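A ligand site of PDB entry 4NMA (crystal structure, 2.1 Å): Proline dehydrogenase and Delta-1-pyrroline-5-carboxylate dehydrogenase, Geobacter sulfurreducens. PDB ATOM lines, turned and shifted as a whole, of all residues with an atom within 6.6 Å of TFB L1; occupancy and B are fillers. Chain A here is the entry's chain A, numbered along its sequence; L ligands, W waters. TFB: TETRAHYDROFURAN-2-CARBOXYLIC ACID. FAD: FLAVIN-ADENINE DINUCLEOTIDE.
The backbone NH (N) of Met 246 lies within hydrogen-bond range of an oxygen (O4) of FAD L2 (3.2 Å). The side-chain amino group (NZ) of Lys 204 lies within salt-bridge range of an oxygen (OXT) of TFB L1 (2.9 Å). The guanidinium group of Arg 304 lies within hydrogen-bond range of a nitrogen (N5) of FAD L2 (3.1 Å). The backbone carbonyl oxygen of Met 246 is in hydrogen-bond range of a nitrogen (N3) of FAD L2 (2.8 Å). The backbone NH (N) of Ala 309 lies within hydrogen-bond range of an oxygen (O2) of FAD L2, 2.9 Å away. The side-chain carboxylate (OE2) of Glu 426 is in hydrogen-bond range of an oxygen (O3') of FAD L2. OB of TFB L1 lies within salt-bridge range of NH1 of Arg 423. The guanidinium group (NE) of Arg 422 is in salt-bridge range of an oxygen (OB) of TFB L1 (2.7 Å). NH2 of Arg 423 is in hydrogen-bond range of O2' of FAD L2, 3.3 Å away.
Water W1 lies within hydrogen-bond range of the side-chain hydroxyl of Tyr 310 (2.6 Å), an oxygen (OA) of TFB L1 (2.7 Å), the backbone carbonyl oxygen of Met 246 (2.9 Å), a nitrogen (N3) of FAD L2 (3.3 Å) and the side-chain amino group of Lys 204 (3.3 Å).
The side-chain carboxylate of Glu 426 lies within salt-bridge range of the guanidinium group of Arg 423, at 2.8 Å. NH1 of Arg 304 lies within salt-bridge range of OD1 of Asp 245. The side-chain hydroxyl (OH) of Tyr 407 is in hydrogen-bond range of the side-chain carboxylate (OD2) of Asp 245 (2.6 Å). The side-chain amino group of Lys 204 lies within salt-bridge range of the side-chain carboxylate of Asp 245 (3.1 Å). The side-chain hydroxyl (OH) of Tyr 407 lies close to the side-chain carboxylate (OD1) of Asp 146. The guanidinium group (NH2) of Arg 422 is in salt-bridge range of the side-chain carboxylate (OE1) of Glu 150 (3.1 Å). NH1 of Arg 422 lies close to O of Gly 418 (3.4 Å). The guanidinium group of Arg 423 sits close to the backbone carbonyl oxygen of Tyr 419 (3.4 Å).
Merely in contact with TFB L1: Asp 245 (3.6 Å), Ala 309 (3.7 Å), Leu 386 (3.7 Å), Tyr 407 (3.3 Å) and Tyr 419 (3.4 Å). Hydrophobic or aromatic side chains that line TFB L1: Ala 309, Leu 386, Tyr 407 and Tyr 419.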
ATOM      1  N   ASP A 146      13.517 -12.680  -2.668  1.00  0.00           N
ATOM      2  CA  ASP A 146      14.543 -13.108  -1.724  1.00  0.00           C
ATOM      3  C   ASP A 146      13.947 -14.087  -0.736  1.00  0.00           C
ATOM      4  O   ASP A 146      12.788 -13.969  -0.355  1.00  0.00           O
ATOM      5  CB  ASP A 146      15.129 -11.909  -0.970  1.00  0.00           C
ATOM      6  CG  ASP A 146      16.063 -12.336   0.157  1.00  0.00           C
ATOM      7  OD1 ASP A 146      17.211 -12.742  -0.144  1.00  0.00           O
ATOM      8  OD2 ASP A 146      15.651 -12.264   1.344  1.00  0.00           O
ATOM      9  N   GLU A 150      20.040 -15.243   6.779  1.00  0.00           N
ATOM     10  CA  GLU A 150      21.439 -14.845   6.641  1.00  0.00           C
ATOM     11  C   GLU A 150      22.198 -15.491   7.793  1.00  0.00           C
ATOM     12  O   GLU A 150      21.576 -15.999   8.729  1.00  0.00           O
ATOM     13  CB  GLU A 150      21.565 -13.329   6.750  1.00  0.00           C
ATOM     14  CG  GLU A 150      21.216 -12.826   8.145  1.00  0.00           C
ATOM     15  CD  GLU A 150      20.401 -11.539   8.143  1.00  0.00           C
ATOM     16  OE1 GLU A 150      19.861 -11.163   7.076  1.00  0.00           O
ATOM     17  OE2 GLU A 150      20.320 -10.901   9.215  1.00  0.00           O
ATOM     18  N   ALA A 202      17.370 -12.473  -5.494  1.00  0.00           N
ATOM     19  CA  ALA A 202      18.556 -12.034  -4.767  1.00  0.00           C
ATOM     20  C   ALA A 202      18.906 -13.081  -3.727  1.00  0.00           C
ATOM     21  O   ALA A 202      18.018 -13.721  -3.147  1.00  0.00           O
ATOM     22  CB  ALA A 202      18.340 -10.665  -4.113  1.00  0.00           C
ATOM     23  N   LYS A 204      21.594 -14.048  -0.343  1.00  0.00           N
ATOM     24  CA  LYS A 204      22.573 -13.601   0.654  1.00  0.00           C
ATOM     25  C   LYS A 204      23.703 -14.620   0.883  1.00  0.00           C
ATOM     26  O   LYS A 204      23.467 -15.719   1.385  1.00  0.00           O
ATOM     27  CB  LYS A 204      21.886 -13.261   1.983  1.00  0.00           C
ATOM     28  CG  LYS A 204      21.256 -11.867   1.992  1.00  0.00           C
ATOM     29  CD  LYS A 204      20.771 -11.508   3.388  1.00  0.00           C
ATOM     30  CE  LYS A 204      20.535 -10.004   3.514  1.00  0.00           C
ATOM     31  NZ  LYS A 204      19.569  -9.525   2.508  1.00  0.00           N
ATOM     32  N   ASP A 245      23.352 -10.032  -3.119  1.00  0.00           N
ATOM     33  CA  ASP A 245      23.248  -9.033  -2.041  1.00  0.00           C
ATOM     34  C   ASP A 245      24.610  -8.799  -1.411  1.00  0.00           C
ATOM     35  O   ASP A 245      25.445  -9.706  -1.383  1.00  0.00           O
ATOM     36  CB  ASP A 245      22.294  -9.520  -0.947  1.00  0.00           C
ATOM     37  CG  ASP A 245      20.819  -9.296  -1.302  1.00  0.00           C
ATOM     38  OD1 ASP A 245      20.518  -8.648  -2.338  1.00  0.00           O
ATOM     39  OD2 ASP A 245      19.960  -9.768  -0.524  1.00  0.00           O
ATOM     40  N   MET A 246      24.811  -7.603  -0.874  1.00  0.00           N
ATOM     41  CA  MET A 246      26.031  -7.288  -0.145  1.00  0.00           C
ATOM     42  C   MET A 246      25.714  -7.220   1.347  1.00  0.00           C
ATOM     43  O   MET A 246      24.691  -6.666   1.774  1.00  0.00           O
ATOM     44  CB  MET A 246      26.618  -5.960  -0.663  1.00  0.00           C
ATOM     45  CG  MET A 246      27.975  -5.577  -0.110  1.00  0.00           C
ATOM     46  SD  MET A 246      29.203  -6.886  -0.269  1.00  0.00           S
ATOM     47  CE  MET A 246      29.717  -6.703  -1.975  1.00  0.00           C
ATOM     48  N   ARG A 304      23.559  -3.080  -8.453  1.00  0.00           N
ATOM     49  CA  ARG A 304      22.535  -2.418  -7.681  1.00  0.00           C
ATOM     50  C   ARG A 304      23.265  -1.523  -6.669  1.00  0.00           C
ATOM     51  O   ARG A 304      23.973  -2.012  -5.786  1.00  0.00           O
ATOM     52  CB  ARG A 304      21.615  -3.413  -6.951  1.00  0.00           C
ATOM     53  CG  ARG A 304      20.486  -2.752  -6.167  1.00  0.00           C
ATOM     54  CD  ARG A 304      19.975  -3.619  -5.005  1.00  0.00           C
ATOM     55  NE  ARG A 304      19.554  -4.946  -5.459  1.00  0.00           N
ATOM     56  CZ  ARG A 304      19.565  -6.035  -4.698  1.00  0.00           C
ATOM     57  NH1 ARG A 304      19.966  -5.983  -3.422  1.00  0.00           N
ATOM     58  NH2 ARG A 304      19.155  -7.187  -5.207  1.00  0.00           N
ATOM     59  N   ALA A 309      22.850  -1.085   4.720  1.00  0.00           N
ATOM     60  CA  ALA A 309      21.888  -1.453   5.758  1.00  0.00           C
ATOM     61  C   ALA A 309      22.482  -1.756   7.152  1.00  0.00           C
ATOM     62  O   ALA A 309      21.719  -2.010   8.088  1.00  0.00           O
ATOM     63  CB  ALA A 309      20.991  -2.621   5.284  1.00  0.00           C
ATOM     64  N   TYR A 310      23.803  -1.707   7.300  1.00  0.00           N
ATOM     65  CA  TYR A 310      24.444  -2.126   8.541  1.00  0.00           C
ATOM     66  C   TYR A 310      25.245  -1.019   9.240  1.00  0.00           C
ATOM     67  O   TYR A 310      26.280  -1.285   9.848  1.00  0.00           O
ATOM     68  CB  TYR A 310      25.364  -3.324   8.275  1.00  0.00           C
ATOM     69  CG  TYR A 310      24.675  -4.423   7.473  1.00  0.00           C
ATOM     70  CD1 TYR A 310      23.873  -5.372   8.102  1.00  0.00           C
ATOM     71  CD2 TYR A 310      24.823  -4.496   6.081  1.00  0.00           C
ATOM     72  CE1 TYR A 310      23.232  -6.374   7.379  1.00  0.00           C
ATOM     73  CE2 TYR A 310      24.183  -5.495   5.349  1.00  0.00           C
ATOM     74  CZ  TYR A 310      23.387  -6.425   6.006  1.00  0.00           C
ATOM     75  OH  TYR A 310      22.756  -7.423   5.286  1.00  0.00           O
ATOM     76  N   LEU A 386      12.157  -1.431  -1.481  1.00  0.00           N
ATOM     77  CA  LEU A 386      11.834  -2.547  -0.600  1.00  0.00           C
ATOM     78  C   LEU A 386      10.313  -2.657  -0.469  1.00  0.00           C
ATOM     79  O   LEU A 386       9.616  -1.655  -0.325  1.00  0.00           O
ATOM     80  CB  LEU A 386      12.480  -2.369   0.773  1.00  0.00           C
ATOM     81  CG  LEU A 386      13.998  -2.279   0.825  1.00  0.00           C
ATOM     82  CD1 LEU A 386      14.473  -1.919   2.225  1.00  0.00           C
ATOM     83  CD2 LEU A 386      14.620  -3.579   0.359  1.00  0.00           C
ATOM     84  N   TYR A 407      11.815  -5.293  -4.065  1.00  0.00           N
ATOM     85  CA  TYR A 407      12.569  -6.333  -3.379  1.00  0.00           C
ATOM     86  C   TYR A 407      11.570  -7.037  -2.470  1.00  0.00           C
ATOM     87  O   TYR A 407      11.109  -6.461  -1.485  1.00  0.00           O
ATOM     88  CB  TYR A 407      13.708  -5.746  -2.563  1.00  0.00           C
ATOM     89  CG  TYR A 407      14.692  -6.757  -1.993  1.00  0.00           C
ATOM     90  CD1 TYR A 407      14.423  -7.408  -0.799  1.00  0.00           C
ATOM     91  CD2 TYR A 407      15.894  -7.043  -2.641  1.00  0.00           C
ATOM     92  CE1 TYR A 407      15.317  -8.329  -0.260  1.00  0.00           C
ATOM     93  CE2 TYR A 407      16.794  -7.969  -2.114  1.00  0.00           C
ATOM     94  CZ  TYR A 407      16.498  -8.612  -0.918  1.00  0.00           C
ATOM     95  OH  TYR A 407      17.378  -9.528  -0.379  1.00  0.00           O
ATOM     96  N   GLY A 418      16.530 -10.240  11.487  1.00  0.00           N
ATOM     97  CA  GLY A 418      17.562  -9.268  11.162  1.00  0.00           C
ATOM     98  C   GLY A 418      17.038  -8.257  10.157  1.00  0.00           C
ATOM     99  O   GLY A 418      17.180  -7.034  10.337  1.00  0.00           O
ATOM    100  N   TYR A 419      16.428  -8.777   9.094  1.00  0.00           N
ATOM    101  CA  TYR A 419      15.800  -7.945   8.071  1.00  0.00           C
ATOM    102  C   TYR A 419      14.699  -7.051   8.672  1.00  0.00           C
ATOM    103  O   TYR A 419      14.652  -5.853   8.390  1.00  0.00           O
ATOM    104  CB  TYR A 419      15.250  -8.826   6.942  1.00  0.00           C
ATOM    105  CG  TYR A 419      14.680  -8.055   5.754  1.00  0.00           C
ATOM    106  CD1 TYR A 419      13.386  -7.576   5.780  1.00  0.00           C
ATOM    107  CD2 TYR A 419      15.451  -7.830   4.617  1.00  0.00           C
ATOM    108  CE1 TYR A 419      12.855  -6.877   4.709  1.00  0.00           C
ATOM    109  CE2 TYR A 419      14.925  -7.137   3.534  1.00  0.00           C
ATOM    110  CZ  TYR A 419      13.627  -6.671   3.598  1.00  0.00           C
ATOM    111  OH  TYR A 419      13.077  -5.987   2.542  1.00  0.00           O
ATOM    112  N   ARG A 422      16.216  -4.276  10.808  1.00  0.00           N
ATOM    113  CA  ARG A 422      16.833  -3.308   9.892  1.00  0.00           C
ATOM    114  C   ARG A 422      15.802  -2.387   9.224  1.00  0.00           C
ATOM    115  O   ARG A 422      16.051  -1.181   9.057  1.00  0.00           O
ATOM    116  CB  ARG A 422      17.718  -3.991   8.856  1.00  0.00           C
ATOM    117  CG  ARG A 422      18.996  -4.561   9.466  1.00  0.00           C
ATOM    118  CD  ARG A 422      20.004  -4.982   8.404  1.00  0.00           C
ATOM    119  NE  ARG A 422      19.492  -6.012   7.492  1.00  0.00           N
ATOM    120  CZ  ARG A 422      19.568  -7.321   7.727  1.00  0.00           C
ATOM    121  NH1 ARG A 422      20.106  -7.776   8.862  1.00  0.00           N
ATOM    122  NH2 ARG A 422      19.091  -8.176   6.847  1.00  0.00           N
ATOM    123  N   ARG A 423      14.647  -2.917   8.861  1.00  0.00           N
ATOM    124  CA  ARG A 423      13.596  -2.064   8.306  1.00  0.00           C
ATOM    125  C   ARG A 423      13.103  -1.046   9.323  1.00  0.00           C
ATOM    126  O   ARG A 423      12.920   0.126   8.999  1.00  0.00           O
ATOM    127  CB  ARG A 423      12.430  -2.888   7.766  1.00  0.00           C
ATOM    128  CG  ARG A 423      12.790  -3.831   6.646  1.00  0.00           C
ATOM    129  CD  ARG A 423      13.202  -3.100   5.364  1.00  0.00           C
ATOM    130  NE  ARG A 423      14.563  -2.559   5.388  1.00  0.00           N
ATOM    131  CZ  ARG A 423      15.678  -3.288   5.366  1.00  0.00           C
ATOM    132  NH1 ARG A 423      15.611  -4.609   5.340  1.00  0.00           N
ATOM    133  NH2 ARG A 423      16.870  -2.692   5.372  1.00  0.00           N
ATOM    134  N   GLU A 426      15.632   1.580   9.876  1.00  0.00           N
ATOM    135  CA  GLU A 426      15.661   2.387   8.670  1.00  0.00           C
ATOM    136  C   GLU A 426      14.587   3.474   8.671  1.00  0.00           C
ATOM    137  O   GLU A 426      14.886   4.636   8.388  1.00  0.00           O
ATOM    138  CB  GLU A 426      15.519   1.486   7.444  1.00  0.00           C
ATOM    139  CG  GLU A 426      15.643   2.203   6.121  1.00  0.00           C
ATOM    140  CD  GLU A 426      15.573   1.271   4.933  1.00  0.00           C
ATOM    141  OE1 GLU A 426      15.694   0.032   5.132  1.00  0.00           O
ATOM    142  OE2 GLU A 426      15.413   1.764   3.804  1.00  0.00           O
HETATM  143  OA  TFB L   1      19.612  -6.413   1.876  1.00  0.00           O
HETATM  144  CA  TFB L   1      19.102  -5.435   2.761  1.00  0.00           C
HETATM  145  C   TFB L   1      18.780  -6.055   4.110  1.00  0.00           C
HETATM  146  OB  TFB L   1      18.491  -5.297   5.110  1.00  0.00           O
HETATM  147  CB  TFB L   1      17.916  -4.857   2.131  1.00  0.00           C
HETATM  148  CG  TFB L   1      17.622  -5.680   0.960  1.00  0.00           C
HETATM  149  CD  TFB L   1      18.586  -6.784   0.975  1.00  0.00           C
HETATM  150  OXT TFB L   1      18.807  -7.327   4.248  1.00  0.00           O
HETATM  151  PA  FAD L   2      17.898   7.560   3.333  1.00  0.00           P
HETATM  152  O1A FAD L   2      17.134   8.126   4.552  1.00  0.00           O
HETATM  153  O2A FAD L   2      18.156   8.489   2.253  1.00  0.00           O
HETATM  154  O5B FAD L   2      19.280   7.084   3.538  1.00  0.00           O
HETATM  155  C5B FAD L   2      19.579   6.373   4.743  1.00  0.00           C
HETATM  156  C4B FAD L   2      20.945   5.685   4.641  1.00  0.00           C
HETATM  157  O4B FAD L   2      22.006   6.572   4.895  1.00  0.00           O
HETATM  158  C3B FAD L   2      21.134   4.562   5.609  1.00  0.00           C
HETATM  159  O3B FAD L   2      20.574   3.371   5.232  1.00  0.00           O
HETATM  160  C2B FAD L   2      22.623   4.468   5.670  1.00  0.00           C
HETATM  161  O2B FAD L   2      23.142   3.712   4.649  1.00  0.00           O
HETATM  162  C1B FAD L   2      23.052   5.882   5.528  1.00  0.00           C
HETATM  163  N9A FAD L   2      23.329   6.557   6.773  1.00  0.00           N
HETATM  164  C8A FAD L   2      22.499   6.723   7.870  1.00  0.00           C
HETATM  165  N7A FAD L   2      23.106   7.427   8.826  1.00  0.00           N
HETATM  166  C5A FAD L   2      24.370   7.773   8.381  1.00  0.00           C
HETATM  167  C6A FAD L   2      25.432   8.505   8.921  1.00  0.00           C
HETATM  168  N6A FAD L   2      25.329   9.082  10.237  1.00  0.00           N
HETATM  169  N1A FAD L   2      26.556   8.669   8.199  1.00  0.00           N
HETATM  170  C2A FAD L   2      26.689   8.130   6.964  1.00  0.00           C
HETATM  171  N3A FAD L   2      25.679   7.420   6.404  1.00  0.00           N
HETATM  172  C4A FAD L   2      24.532   7.239   7.065  1.00  0.00           C
HETATM  173  N1  FAD L   2      21.903  -2.399   1.749  1.00  0.00           N
HETATM  174  C2  FAD L   2      22.921  -3.395   1.976  1.00  0.00           C
HETATM  175  O2  FAD L   2      23.852  -3.158   2.918  1.00  0.00           O
HETATM  176  N3  FAD L   2      22.980  -4.556   1.242  1.00  0.00           N
HETATM  177  C4  FAD L   2      22.020  -4.814   0.279  1.00  0.00           C
HETATM  178  O4  FAD L   2      22.062  -5.956  -0.472  1.00  0.00           O
HETATM  179  C4X FAD L   2      20.921  -3.855   0.032  1.00  0.00           C
HETATM  180  N5  FAD L   2      19.941  -4.105  -0.919  1.00  0.00           N
HETATM  181  C5X FAD L   2      18.936  -3.159  -1.151  1.00  0.00           C
HETATM  182  C6  FAD L   2      17.948  -3.433  -2.111  1.00  0.00           C
HETATM  183  C7  FAD L   2      16.937  -2.503  -2.339  1.00  0.00           C
HETATM  184  C7M FAD L   2      15.880  -2.779  -3.380  1.00  0.00           C
HETATM  185  C8  FAD L   2      16.895  -1.312  -1.635  1.00  0.00           C
HETATM  186  C8M FAD L   2      15.803  -0.331  -1.905  1.00  0.00           C
HETATM  187  C9  FAD L   2      17.878  -1.033  -0.663  1.00  0.00           C
HETATM  188  C9A FAD L   2      18.896  -1.962  -0.423  1.00  0.00           C
HETATM  189  N10 FAD L   2      19.903  -1.701   0.576  1.00  0.00           N
HETATM  190  C10 FAD L   2      20.919  -2.636   0.792  1.00  0.00           C
HETATM  191  C1' FAD L   2      19.905  -0.423   1.304  1.00  0.00           C
HETATM  192  C2' FAD L   2      19.278  -0.474   2.673  1.00  0.00           C
HETATM  193  O2' FAD L   2      18.477  -1.587   2.747  1.00  0.00           O
HETATM  194  C3' FAD L   2      18.439   0.795   2.885  1.00  0.00           C
HETATM  195  O3' FAD L   2      17.252   0.575   2.213  1.00  0.00           O
HETATM  196  C4' FAD L   2      19.074   2.090   2.371  1.00  0.00           C
HETATM  197  O4' FAD L   2      20.370   2.199   2.824  1.00  0.00           O
HETATM  198  C5' FAD L   2      18.274   3.354   2.712  1.00  0.00           C
HETATM  199  O5' FAD L   2      18.692   4.415   1.874  1.00  0.00           O
HETATM  200  P   FAD L   2      17.751   5.583   1.289  1.00  0.00           P
HETATM  201  O1P FAD L   2      18.228   6.328  -0.003  1.00  0.00           O
HETATM  202  O2P FAD L   2      16.463   4.699   1.164  1.00  0.00           O
HETATM  203  O3P FAD L   2      17.248   6.414   2.602  1.00  0.00           O
HETATM  204  O   HOH W   1      22.051  -7.296   2.770  1.00  0.00           O
